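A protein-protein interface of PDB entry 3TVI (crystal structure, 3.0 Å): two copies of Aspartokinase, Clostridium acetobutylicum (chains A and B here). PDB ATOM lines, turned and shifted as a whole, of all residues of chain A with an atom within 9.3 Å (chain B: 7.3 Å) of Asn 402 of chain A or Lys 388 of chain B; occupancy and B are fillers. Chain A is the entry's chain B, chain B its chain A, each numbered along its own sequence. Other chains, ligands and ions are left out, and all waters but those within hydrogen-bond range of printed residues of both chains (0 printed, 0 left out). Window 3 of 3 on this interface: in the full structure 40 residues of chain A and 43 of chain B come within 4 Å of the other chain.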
ATOM      1  N   PHE A 395       0.192  -0.165  -7.659  1.00  0.00           N
ATOM      2  CA  PHE A 395       1.336  -1.039  -7.456  1.00  0.00           C
ATOM      3  C   PHE A 395       2.523  -0.255  -6.923  1.00  0.00           C
ATOM      4  O   PHE A 395       3.315  -0.796  -6.149  1.00  0.00           O
ATOM      5  CB  PHE A 395       1.706  -1.769  -8.741  1.00  0.00           C
ATOM      6  CG  PHE A 395       0.547  -2.469  -9.389  1.00  0.00           C
ATOM      7  CD1 PHE A 395      -0.332  -3.226  -8.634  1.00  0.00           C
ATOM      8  CD2 PHE A 395       0.339  -2.377 -10.756  1.00  0.00           C
ATOM      9  CE1 PHE A 395      -1.403  -3.872  -9.227  1.00  0.00           C
ATOM     10  CE2 PHE A 395      -0.735  -3.014 -11.356  1.00  0.00           C
ATOM     11  CZ  PHE A 395      -1.606  -3.766 -10.590  1.00  0.00           C
ATOM     12  N   THR A 396       2.640   1.011  -7.326  1.00  0.00           N
ATOM     13  CA  THR A 396       3.669   1.880  -6.778  1.00  0.00           C
ATOM     14  C   THR A 396       3.435   1.989  -5.298  1.00  0.00           C
ATOM     15  O   THR A 396       4.343   1.770  -4.518  1.00  0.00           O
ATOM     16  CB  THR A 396       3.652   3.305  -7.353  1.00  0.00           C
ATOM     17  OG1 THR A 396       3.542   3.265  -8.776  1.00  0.00           O
ATOM     18  CG2 THR A 396       4.930   4.031  -6.975  1.00  0.00           C
ATOM     19  N   ALA A 397       2.210   2.320  -4.916  1.00  0.00           N
ATOM     20  CA  ALA A 397       1.849   2.403  -3.508  1.00  0.00           C
ATOM     21  C   ALA A 397       2.311   1.156  -2.778  1.00  0.00           C
ATOM     22  O   ALA A 397       3.095   1.244  -1.833  1.00  0.00           O
ATOM     23  CB  ALA A 397       0.347   2.573  -3.347  1.00  0.00           C
ATOM     24  N   LEU A 398       1.846  -0.005  -3.238  1.00  0.00           N
ATOM     25  CA  LEU A 398       2.157  -1.278  -2.576  1.00  0.00           C
ATOM     26  C   LEU A 398       3.654  -1.585  -2.559  1.00  0.00           C
ATOM     27  O   LEU A 398       4.131  -2.230  -1.635  1.00  0.00           O
ATOM     28  CB  LEU A 398       1.399  -2.434  -3.228  1.00  0.00           C
ATOM     29  CG  LEU A 398      -0.128  -2.360  -3.190  1.00  0.00           C
ATOM     30  CD1 LEU A 398      -0.732  -3.341  -4.180  1.00  0.00           C
ATOM     31  CD2 LEU A 398      -0.648  -2.621  -1.784  1.00  0.00           C
ATOM     32  N   SER A 399       4.389  -1.133  -3.571  1.00  0.00           N
ATOM     33  CA  SER A 399       5.847  -1.274  -3.576  1.00  0.00           C
ATOM     34  C   SER A 399       6.477  -0.458  -2.458  1.00  0.00           C
ATOM     35  O   SER A 399       7.405  -0.923  -1.798  1.00  0.00           O
ATOM     36  CB  SER A 399       6.452  -0.824  -4.908  1.00  0.00           C
ATOM     37  OG  SER A 399       5.997  -1.623  -5.983  1.00  0.00           O
ATOM     38  N   LYS A 400       5.975   0.759  -2.250  1.00  0.00           N
ATOM     39  CA  LYS A 400       6.517   1.645  -1.214  1.00  0.00           C
ATOM     40  C   LYS A 400       6.351   1.073   0.189  1.00  0.00           C
ATOM     41  O   LYS A 400       7.167   1.346   1.061  1.00  0.00           O
ATOM     42  CB  LYS A 400       5.896   3.046  -1.289  1.00  0.00           C
ATOM     43  CG  LYS A 400       6.681   4.017  -2.154  1.00  0.00           C
ATOM     44  CD  LYS A 400       6.813   3.528  -3.597  1.00  0.00           C
ATOM     45  CE  LYS A 400       7.434   4.581  -4.515  1.00  0.00           C
ATOM     46  NZ  LYS A 400       7.889   4.022  -5.826  1.00  0.00           N
ATOM     47  N   GLU A 401       5.305   0.279   0.402  1.00  0.00           N
ATOM     48  CA  GLU A 401       5.078  -0.365   1.697  1.00  0.00           C
ATOM     49  C   GLU A 401       5.627  -1.789   1.752  1.00  0.00           C
ATOM     50  O   GLU A 401       5.357  -2.528   2.708  1.00  0.00           O
ATOM     51  CB  GLU A 401       3.585  -0.330   2.067  1.00  0.00           C
ATOM     52  CG  GLU A 401       3.217   0.766   3.062  1.00  0.00           C
ATOM     53  CD  GLU A 401       3.994   2.053   2.836  1.00  0.00           C
ATOM     54  OE1 GLU A 401       4.612   2.545   3.805  1.00  0.00           O
ATOM     55  OE2 GLU A 401       4.013   2.554   1.688  1.00  0.00           O
ATOM     56  N   ASN A 402       6.418  -2.156   0.746  1.00  0.00           N
ATOM     57  CA  ASN A 402       7.099  -3.437   0.729  1.00  0.00           C
ATOM     58  C   ASN A 402       6.111  -4.580   0.972  1.00  0.00           C
ATOM     59  O   ASN A 402       6.217  -5.312   1.963  1.00  0.00           O
ATOM     60  CB  ASN A 402       8.232  -3.437   1.772  1.00  0.00           C
ATOM     61  CG  ASN A 402       9.118  -4.672   1.689  1.00  0.00           C
ATOM     62  OD1 ASN A 402       9.457  -5.270   2.712  1.00  0.00           O
ATOM     63  ND2 ASN A 402       9.498  -5.061   0.472  1.00  0.00           N
ATOM     64  N   VAL A 403       5.140  -4.706   0.067  1.00  0.00           N
ATOM     65  CA  VAL A 403       4.098  -5.737   0.174  1.00  0.00           C
ATOM     66  C   VAL A 403       3.911  -6.491  -1.150  1.00  0.00           C
ATOM     67  O   VAL A 403       3.529  -5.922  -2.172  1.00  0.00           O
ATOM     68  CB  VAL A 403       2.751  -5.175   0.714  1.00  0.00           C
ATOM     69  CG1 VAL A 403       2.597  -3.695   0.395  1.00  0.00           C
ATOM     70  CG2 VAL A 403       1.564  -5.988   0.202  1.00  0.00           C
ATOM     71  N   ASN A 404       4.211  -7.785  -1.092  1.00  0.00           N
ATOM     72  CA  ASN A 404       4.133  -8.695  -2.229  1.00  0.00           C
ATOM     73  C   ASN A 404       2.685  -8.879  -2.685  1.00  0.00           C
ATOM     74  O   ASN A 404       1.789  -9.143  -1.866  1.00  0.00           O
ATOM     75  CB  ASN A 404       4.761 -10.049  -1.840  1.00  0.00           C
ATOM     76  CG  ASN A 404       4.410 -11.172  -2.801  1.00  0.00           C
ATOM     77  OD1 ASN A 404       4.986 -11.278  -3.881  1.00  0.00           O
ATOM     78  ND2 ASN A 404       3.482 -12.036  -2.391  1.00  0.00           N
ATOM     79  N   ILE A 405       2.485  -8.729  -3.996  1.00  0.00           N
ATOM     80  CA  ILE A 405       1.192  -8.897  -4.639  1.00  0.00           C
ATOM     81  C   ILE A 405       0.998 -10.367  -4.981  1.00  0.00           C
ATOM     82  O   ILE A 405       1.913 -11.015  -5.472  1.00  0.00           O
ATOM     83  CB  ILE A 405       1.125  -8.057  -5.931  1.00  0.00           C
ATOM     84  CG1 ILE A 405       1.329  -6.573  -5.613  1.00  0.00           C
ATOM     85  CG2 ILE A 405      -0.202  -8.251  -6.652  1.00  0.00           C
ATOM     86  CD1 ILE A 405       1.397  -5.691  -6.840  1.00  0.00           C
ATOM     87  N   VAL A 421      -3.447 -10.032  -1.767  1.00  0.00           N
ATOM     88  CA  VAL A 421      -2.216  -9.966  -0.978  1.00  0.00           C
ATOM     89  C   VAL A 421      -2.294 -10.822   0.269  1.00  0.00           C
ATOM     90  O   VAL A 421      -3.386 -11.187   0.713  1.00  0.00           O
ATOM     91  CB  VAL A 421      -1.930  -8.531  -0.497  1.00  0.00           C
ATOM     92  CG1 VAL A 421      -1.692  -7.611  -1.681  1.00  0.00           C
ATOM     93  CG2 VAL A 421      -3.070  -8.027   0.388  1.00  0.00           C
ATOM     94  N   GLU A 422      -1.124 -11.094   0.849  1.00  0.00           N
ATOM     95  CA  GLU A 422      -1.015 -11.811   2.123  1.00  0.00           C
ATOM     96  C   GLU A 422      -1.890 -11.168   3.189  1.00  0.00           C
ATOM     97  O   GLU A 422      -1.892  -9.943   3.339  1.00  0.00           O
ATOM     98  CB  GLU A 422       0.432 -11.802   2.624  1.00  0.00           C
ATOM     99  CG  GLU A 422       0.867 -13.100   3.287  1.00  0.00           C
ATOM    100  CD  GLU A 422       1.109 -14.209   2.274  1.00  0.00           C
ATOM    101  OE1 GLU A 422       1.902 -14.001   1.317  1.00  0.00           O
ATOM    102  OE2 GLU A 422       0.497 -15.288   2.439  1.00  0.00           O
ATOM    103  N   VAL A 424      -1.598 -10.871   6.302  1.00  0.00           N
ATOM    104  CA  VAL A 424      -0.838  -9.997   7.197  1.00  0.00           C
ATOM    105  C   VAL A 424      -0.753  -8.562   6.656  1.00  0.00           C
ATOM    106  O   VAL A 424      -0.867  -7.600   7.417  1.00  0.00           O
ATOM    107  CB  VAL A 424       0.585 -10.542   7.463  1.00  0.00           C
ATOM    108  CG1 VAL A 424       1.410 -10.588   6.185  1.00  0.00           C
ATOM    109  CG2 VAL A 424       1.284  -9.698   8.521  1.00  0.00           C
ATOM    110  N   ASP A 425      -0.580  -8.432   5.340  1.00  0.00           N
ATOM    111  CA  ASP A 425      -0.389  -7.124   4.689  1.00  0.00           C
ATOM    112  C   ASP A 425      -1.693  -6.367   4.348  1.00  0.00           C
ATOM    113  O   ASP A 425      -1.646  -5.216   3.910  1.00  0.00           O
ATOM    114  CB  ASP A 425       0.463  -7.297   3.422  1.00  0.00           C
ATOM    115  CG  ASP A 425       1.928  -7.598   3.729  1.00  0.00           C
ATOM    116  OD1 ASP A 425       2.333  -7.525   4.913  1.00  0.00           O
ATOM    117  OD2 ASP A 425       2.690  -7.898   2.782  1.00  0.00           O
ATOM    118  N   LYS A 428      -2.062  -2.932   5.704  1.00  0.00           N
ATOM    119  CA  LYS A 428      -0.946  -2.117   5.213  1.00  0.00           C
ATOM    120  C   LYS A 428      -1.236  -1.627   3.795  1.00  0.00           C
ATOM    121  O   LYS A 428      -1.046  -0.454   3.473  1.00  0.00           O
ATOM    122  CB  LYS A 428       0.350  -2.938   5.236  1.00  0.00           C
ATOM    123  CG  LYS A 428       1.638  -2.136   5.336  1.00  0.00           C
ATOM    124  CD  LYS A 428       2.811  -3.080   5.590  1.00  0.00           C
ATOM    125  CE  LYS A 428       4.152  -2.361   5.649  1.00  0.00           C
ATOM    126  NZ  LYS A 428       5.297  -3.277   5.372  1.00  0.00           N
ATOM    127  N   ALA A 429      -1.710  -2.544   2.960  1.00  0.00           N
ATOM    128  CA  ALA A 429      -2.064  -2.238   1.587  1.00  0.00           C
ATOM    129  C   ALA A 429      -3.127  -1.143   1.529  1.00  0.00           C
ATOM    130  O   ALA A 429      -2.894  -0.070   0.966  1.00  0.00           O
ATOM    131  CB  ALA A 429      -2.565  -3.497   0.900  1.00  0.00           C
ATOM    132  N   SER A 432      -1.911   2.146   2.259  1.00  0.00           N
ATOM    133  CA  SER A 432      -1.039   2.664   1.202  1.00  0.00           C
ATOM    134  C   SER A 432      -1.809   3.250   0.037  1.00  0.00           C
ATOM    135  O   SER A 432      -1.422   4.274  -0.521  1.00  0.00           O
ATOM    136  CB  SER A 432      -0.140   1.550   0.659  1.00  0.00           C
ATOM    137  OG  SER A 432       0.021   0.516   1.614  1.00  0.00           O
ATOM    138  N   GLY B 287      14.246 -10.431  -8.682  1.00  0.00           N
ATOM    139  CA  GLY B 287      14.098  -9.215  -9.484  1.00  0.00           C
ATOM    140  C   GLY B 287      14.486  -9.362 -10.953  1.00  0.00           C
ATOM    141  O   GLY B 287      14.818  -8.370 -11.607  1.00  0.00           O
ATOM    142  N   MET B 384      10.690 -13.481 -10.264  1.00  0.00           N
ATOM    143  CA  MET B 384       9.651 -12.528  -9.869  1.00  0.00           C
ATOM    144  C   MET B 384       8.708 -13.247  -8.941  1.00  0.00           C
ATOM    145  O   MET B 384       7.498 -13.086  -9.026  1.00  0.00           O
ATOM    146  CB  MET B 384       8.954 -11.911 -11.095  1.00  0.00           C
ATOM    147  CG  MET B 384       8.632 -12.867 -12.238  1.00  0.00           C
ATOM    148  SD  MET B 384       7.698 -11.926 -13.688  1.00  0.00           S
ATOM    149  CE  MET B 384       6.894 -13.574 -14.355  1.00  0.00           C
ATOM    150  N   ALA B 385       9.267 -14.027  -8.021  1.00  0.00           N
ATOM    151  CA  ALA B 385       8.487 -14.943  -7.203  1.00  0.00           C
ATOM    152  C   ALA B 385       7.774 -14.172  -6.123  1.00  0.00           C
ATOM    153  O   ALA B 385       6.629 -13.778  -6.307  1.00  0.00           O
ATOM    154  CB  ALA B 385       9.386 -16.011  -6.595  1.00  0.00           C
ATOM    155  N   LYS B 386       8.452 -13.943  -5.005  1.00  0.00           N
ATOM    156  CA  LYS B 386       7.884 -13.194  -3.892  1.00  0.00           C
ATOM    157  C   LYS B 386       8.433 -11.772  -3.898  1.00  0.00           C
ATOM    158  O   LYS B 386       8.295 -11.050  -2.913  1.00  0.00           O
ATOM    159  CB  LYS B 386       8.218 -13.878  -2.560  1.00  0.00           C
ATOM    160  CG  LYS B 386       7.177 -14.870  -2.063  1.00  0.00           C
ATOM    161  CD  LYS B 386       7.241 -16.212  -2.774  1.00  0.00           C
ATOM    162  CE  LYS B 386       6.463 -17.281  -2.011  1.00  0.00           C
ATOM    163  NZ  LYS B 386       6.698 -18.655  -2.540  1.00  0.00           N
ATOM    164  N   THR B 387       9.047 -11.369  -5.011  1.00  0.00           N
ATOM    165  CA  THR B 387       9.746 -10.089  -5.085  1.00  0.00           C
ATOM    166  C   THR B 387       8.765  -8.929  -5.227  1.00  0.00           C
ATOM    167  O   THR B 387       7.821  -9.012  -5.998  1.00  0.00           O
ATOM    168  CB  THR B 387      10.718 -10.055  -6.283  1.00  0.00           C
ATOM    169  OG1 THR B 387      11.197 -11.380  -6.558  1.00  0.00           O
ATOM    170  CG2 THR B 387      11.890  -9.124  -5.992  1.00  0.00           C
ATOM    171  N   LYS B 388       8.993  -7.852  -4.480  1.00  0.00           N
ATOM    172  CA  LYS B 388       8.168  -6.652  -4.587  1.00  0.00           C
ATOM    173  C   LYS B 388       8.517  -5.893  -5.861  1.00  0.00           C
ATOM    174  O   LYS B 388       9.648  -5.962  -6.339  1.00  0.00           O
ATOM    175  CB  LYS B 388       8.351  -5.731  -3.367  1.00  0.00           C
ATOM    176  CG  LYS B 388       9.746  -5.122  -3.202  1.00  0.00           C
ATOM    177  CD  LYS B 388       9.731  -3.858  -2.343  1.00  0.00           C
ATOM    178  CE  LYS B 388       9.790  -2.569  -3.156  1.00  0.00           C
ATOM    179  NZ  LYS B 388      11.072  -1.836  -2.966  1.00  0.00           N
ATOM    180  N   GLY B 389       7.535  -5.184  -6.409  1.00  0.00           N
ATOM    181  CA  GLY B 389       7.770  -4.221  -7.483  1.00  0.00           C
ATOM    182  C   GLY B 389       7.868  -4.751  -8.904  1.00  0.00           C
ATOM    183  O   GLY B 389       8.055  -3.971  -9.833  1.00  0.00           O
ATOM    184  N   ILE B 390       7.738  -6.058  -9.096  1.00  0.00           N
ATOM    185  CA  ILE B 390       7.859  -6.625 -10.437  1.00  0.00           C
ATOM    186  C   ILE B 390       6.714  -6.145 -11.320  1.00  0.00           C
ATOM    187  O   ILE B 390       6.936  -5.635 -12.409  1.00  0.00           O
ATOM    188  CB  ILE B 390       7.936  -8.160 -10.390  1.00  0.00           C
ATOM    189  CG1 ILE B 390       9.262  -8.578  -9.763  1.00  0.00           C
ATOM    190  CG2 ILE B 390       7.834  -8.755 -11.782  1.00  0.00           C
ATOM    191  CD1 ILE B 390      10.479  -8.106 -10.541  1.00  0.00           C
ATOM    192  N   ALA B 391       5.492  -6.299 -10.839  1.00  0.00           N
ATOM    193  CA  ALA B 391       4.347  -5.671 -11.469  1.00  0.00           C
ATOM    194  C   ALA B 391       4.686  -4.222 -11.732  1.00  0.00           C
ATOM    195  O   ALA B 391       4.661  -3.754 -12.875  1.00  0.00           O
ATOM    196  CB  ALA B 391       3.135  -5.744 -10.552  1.00  0.00           C
ATOM    197  N   ASN B 392       5.028  -3.523 -10.655  1.00  0.00           N
ATOM    198  CA  ASN B 392       5.238  -2.084 -10.708  1.00  0.00           C
ATOM    199  C   ASN B 392       6.310  -1.699 -11.717  1.00  0.00           C
ATOM    200  O   ASN B 392       6.195  -0.659 -12.367  1.00  0.00           O
ATOM    201  CB  ASN B 392       5.599  -1.547  -9.315  1.00  0.00           C
ATOM    202  CG  ASN B 392       5.570  -0.031  -9.239  1.00  0.00           C
ATOM    203  OD1 ASN B 392       4.842   0.628  -9.982  1.00  0.00           O
ATOM    204  ND2 ASN B 392       6.367   0.529  -8.331  1.00  0.00           N
ATOM    205  N   LYS B 393       7.336  -2.540 -11.859  1.00  0.00           N
ATOM    206  CA  LYS B 393       8.412  -2.287 -12.827  1.00  0.00           C
ATOM    207  C   LYS B 393       7.897  -2.432 -14.253  1.00  0.00           C
ATOM    208  O   LYS B 393       8.175  -1.589 -15.109  1.00  0.00           O
ATOM    209  CB  LYS B 393       9.598  -3.222 -12.610  1.00  0.00           C
ATOM    210  CG  LYS B 393      10.851  -2.701 -13.284  1.00  0.00           C
ATOM    211  CD  LYS B 393      12.065  -3.613 -13.154  1.00  0.00           C
ATOM    212  CE  LYS B 393      13.279  -2.922 -13.761  1.00  0.00           C
ATOM    213  NZ  LYS B 393      14.361  -3.853 -14.177  1.00  0.00           N
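C of Phe 395 of chain A touches CG of Asn 392 of chain B, at 3.8 Å. Lys 388 of chain B touches Ser 399 of chain A. OG of Ser 399 of chain A touches CA of Gly 389 of chain B (3.5 Å). ND2 of Asn 402 of chain A touches CD of Lys 388 of chain B, 3.1 Å away. OD1 of Asn 404 of chain A touches O of Ala 385 of chain B, at 3.9 Å.
Asn 402 of chain A touches one residue of chain B. Lys 388 of chain B touches just these residues of chain A: Ser 399 (3.2 Å) and Asn 402 (3.1 Å). No residue of chain A comes within 4 Å of Thr 387 of chain B. Of chain A, only Ser 399 (3.5 Å) comes within 4 Å of Gly 389 of chain B. Printed residues of chain B within 4 Å of Asn 404 of chain A: Ala 385 (3.9 Å) and Lys 386 (3.5 Å). Of the printed residues of chain B, Thr 396 of chain A touches Asn 392 (3.2 Å). Printed residues of chain B within 4 Å of Phe 395 of chain A: Asn 392 (3.8 Å). Printed residues of chain A within 4 Å of Lys 386 of chain B: Asn 404 (3.5 Å). Of the printed residues of chain B, Ser 399 of chain A touches Lys 388, Gly 389 and Asn 392. Met 384 of chain B touches none of the printed residues of chain A. The nearest residue of chain A that does not touch Lys 388 of chain B is Val 403 of chain A (4.8 Å). The nearest printed residue of chain B that does not touch Thr 396 of chain A is Lys 388 of chain B (7.1 Å).
The backbone carbonyl oxygen (O) of Lys 386 of chain B sits close to the side-chain amide oxygen (OD1) of Asn 404 of chain A, 3.5 Å away. The side-chain amide oxygen (OD1) of Asn 392 of chain B is in hydrogen-bond range of the side-chain hydroxyl (OG1) of Thr 396 of chain A (3.2 Å). OG of Ser 399 of chain A is in hydrogen-bond range of ND2 of Asn 392 of chain B, 3.2 Å away.
No position is printed for both chains.
The side-chain hydroxyl (OG) of Ser 399 of chain A lies within hydrogen-bond range of the backbone carbonyl oxygen (O) of Phe 395 of chain A.
Of the 18 printed residues of chain A, 5 touch a printed residue of chain B. Hydrophobic or aromatic side chains of chain A that line the printed part of chain B: Phe 395. Of the 11 printed residues of chain B, 5 touch a printed residue of chain A. Among the printed residues, no Asp or Glu carboxylate lies within 4 Å of a Lys or Arg side-chain nitrogen of the other chain.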
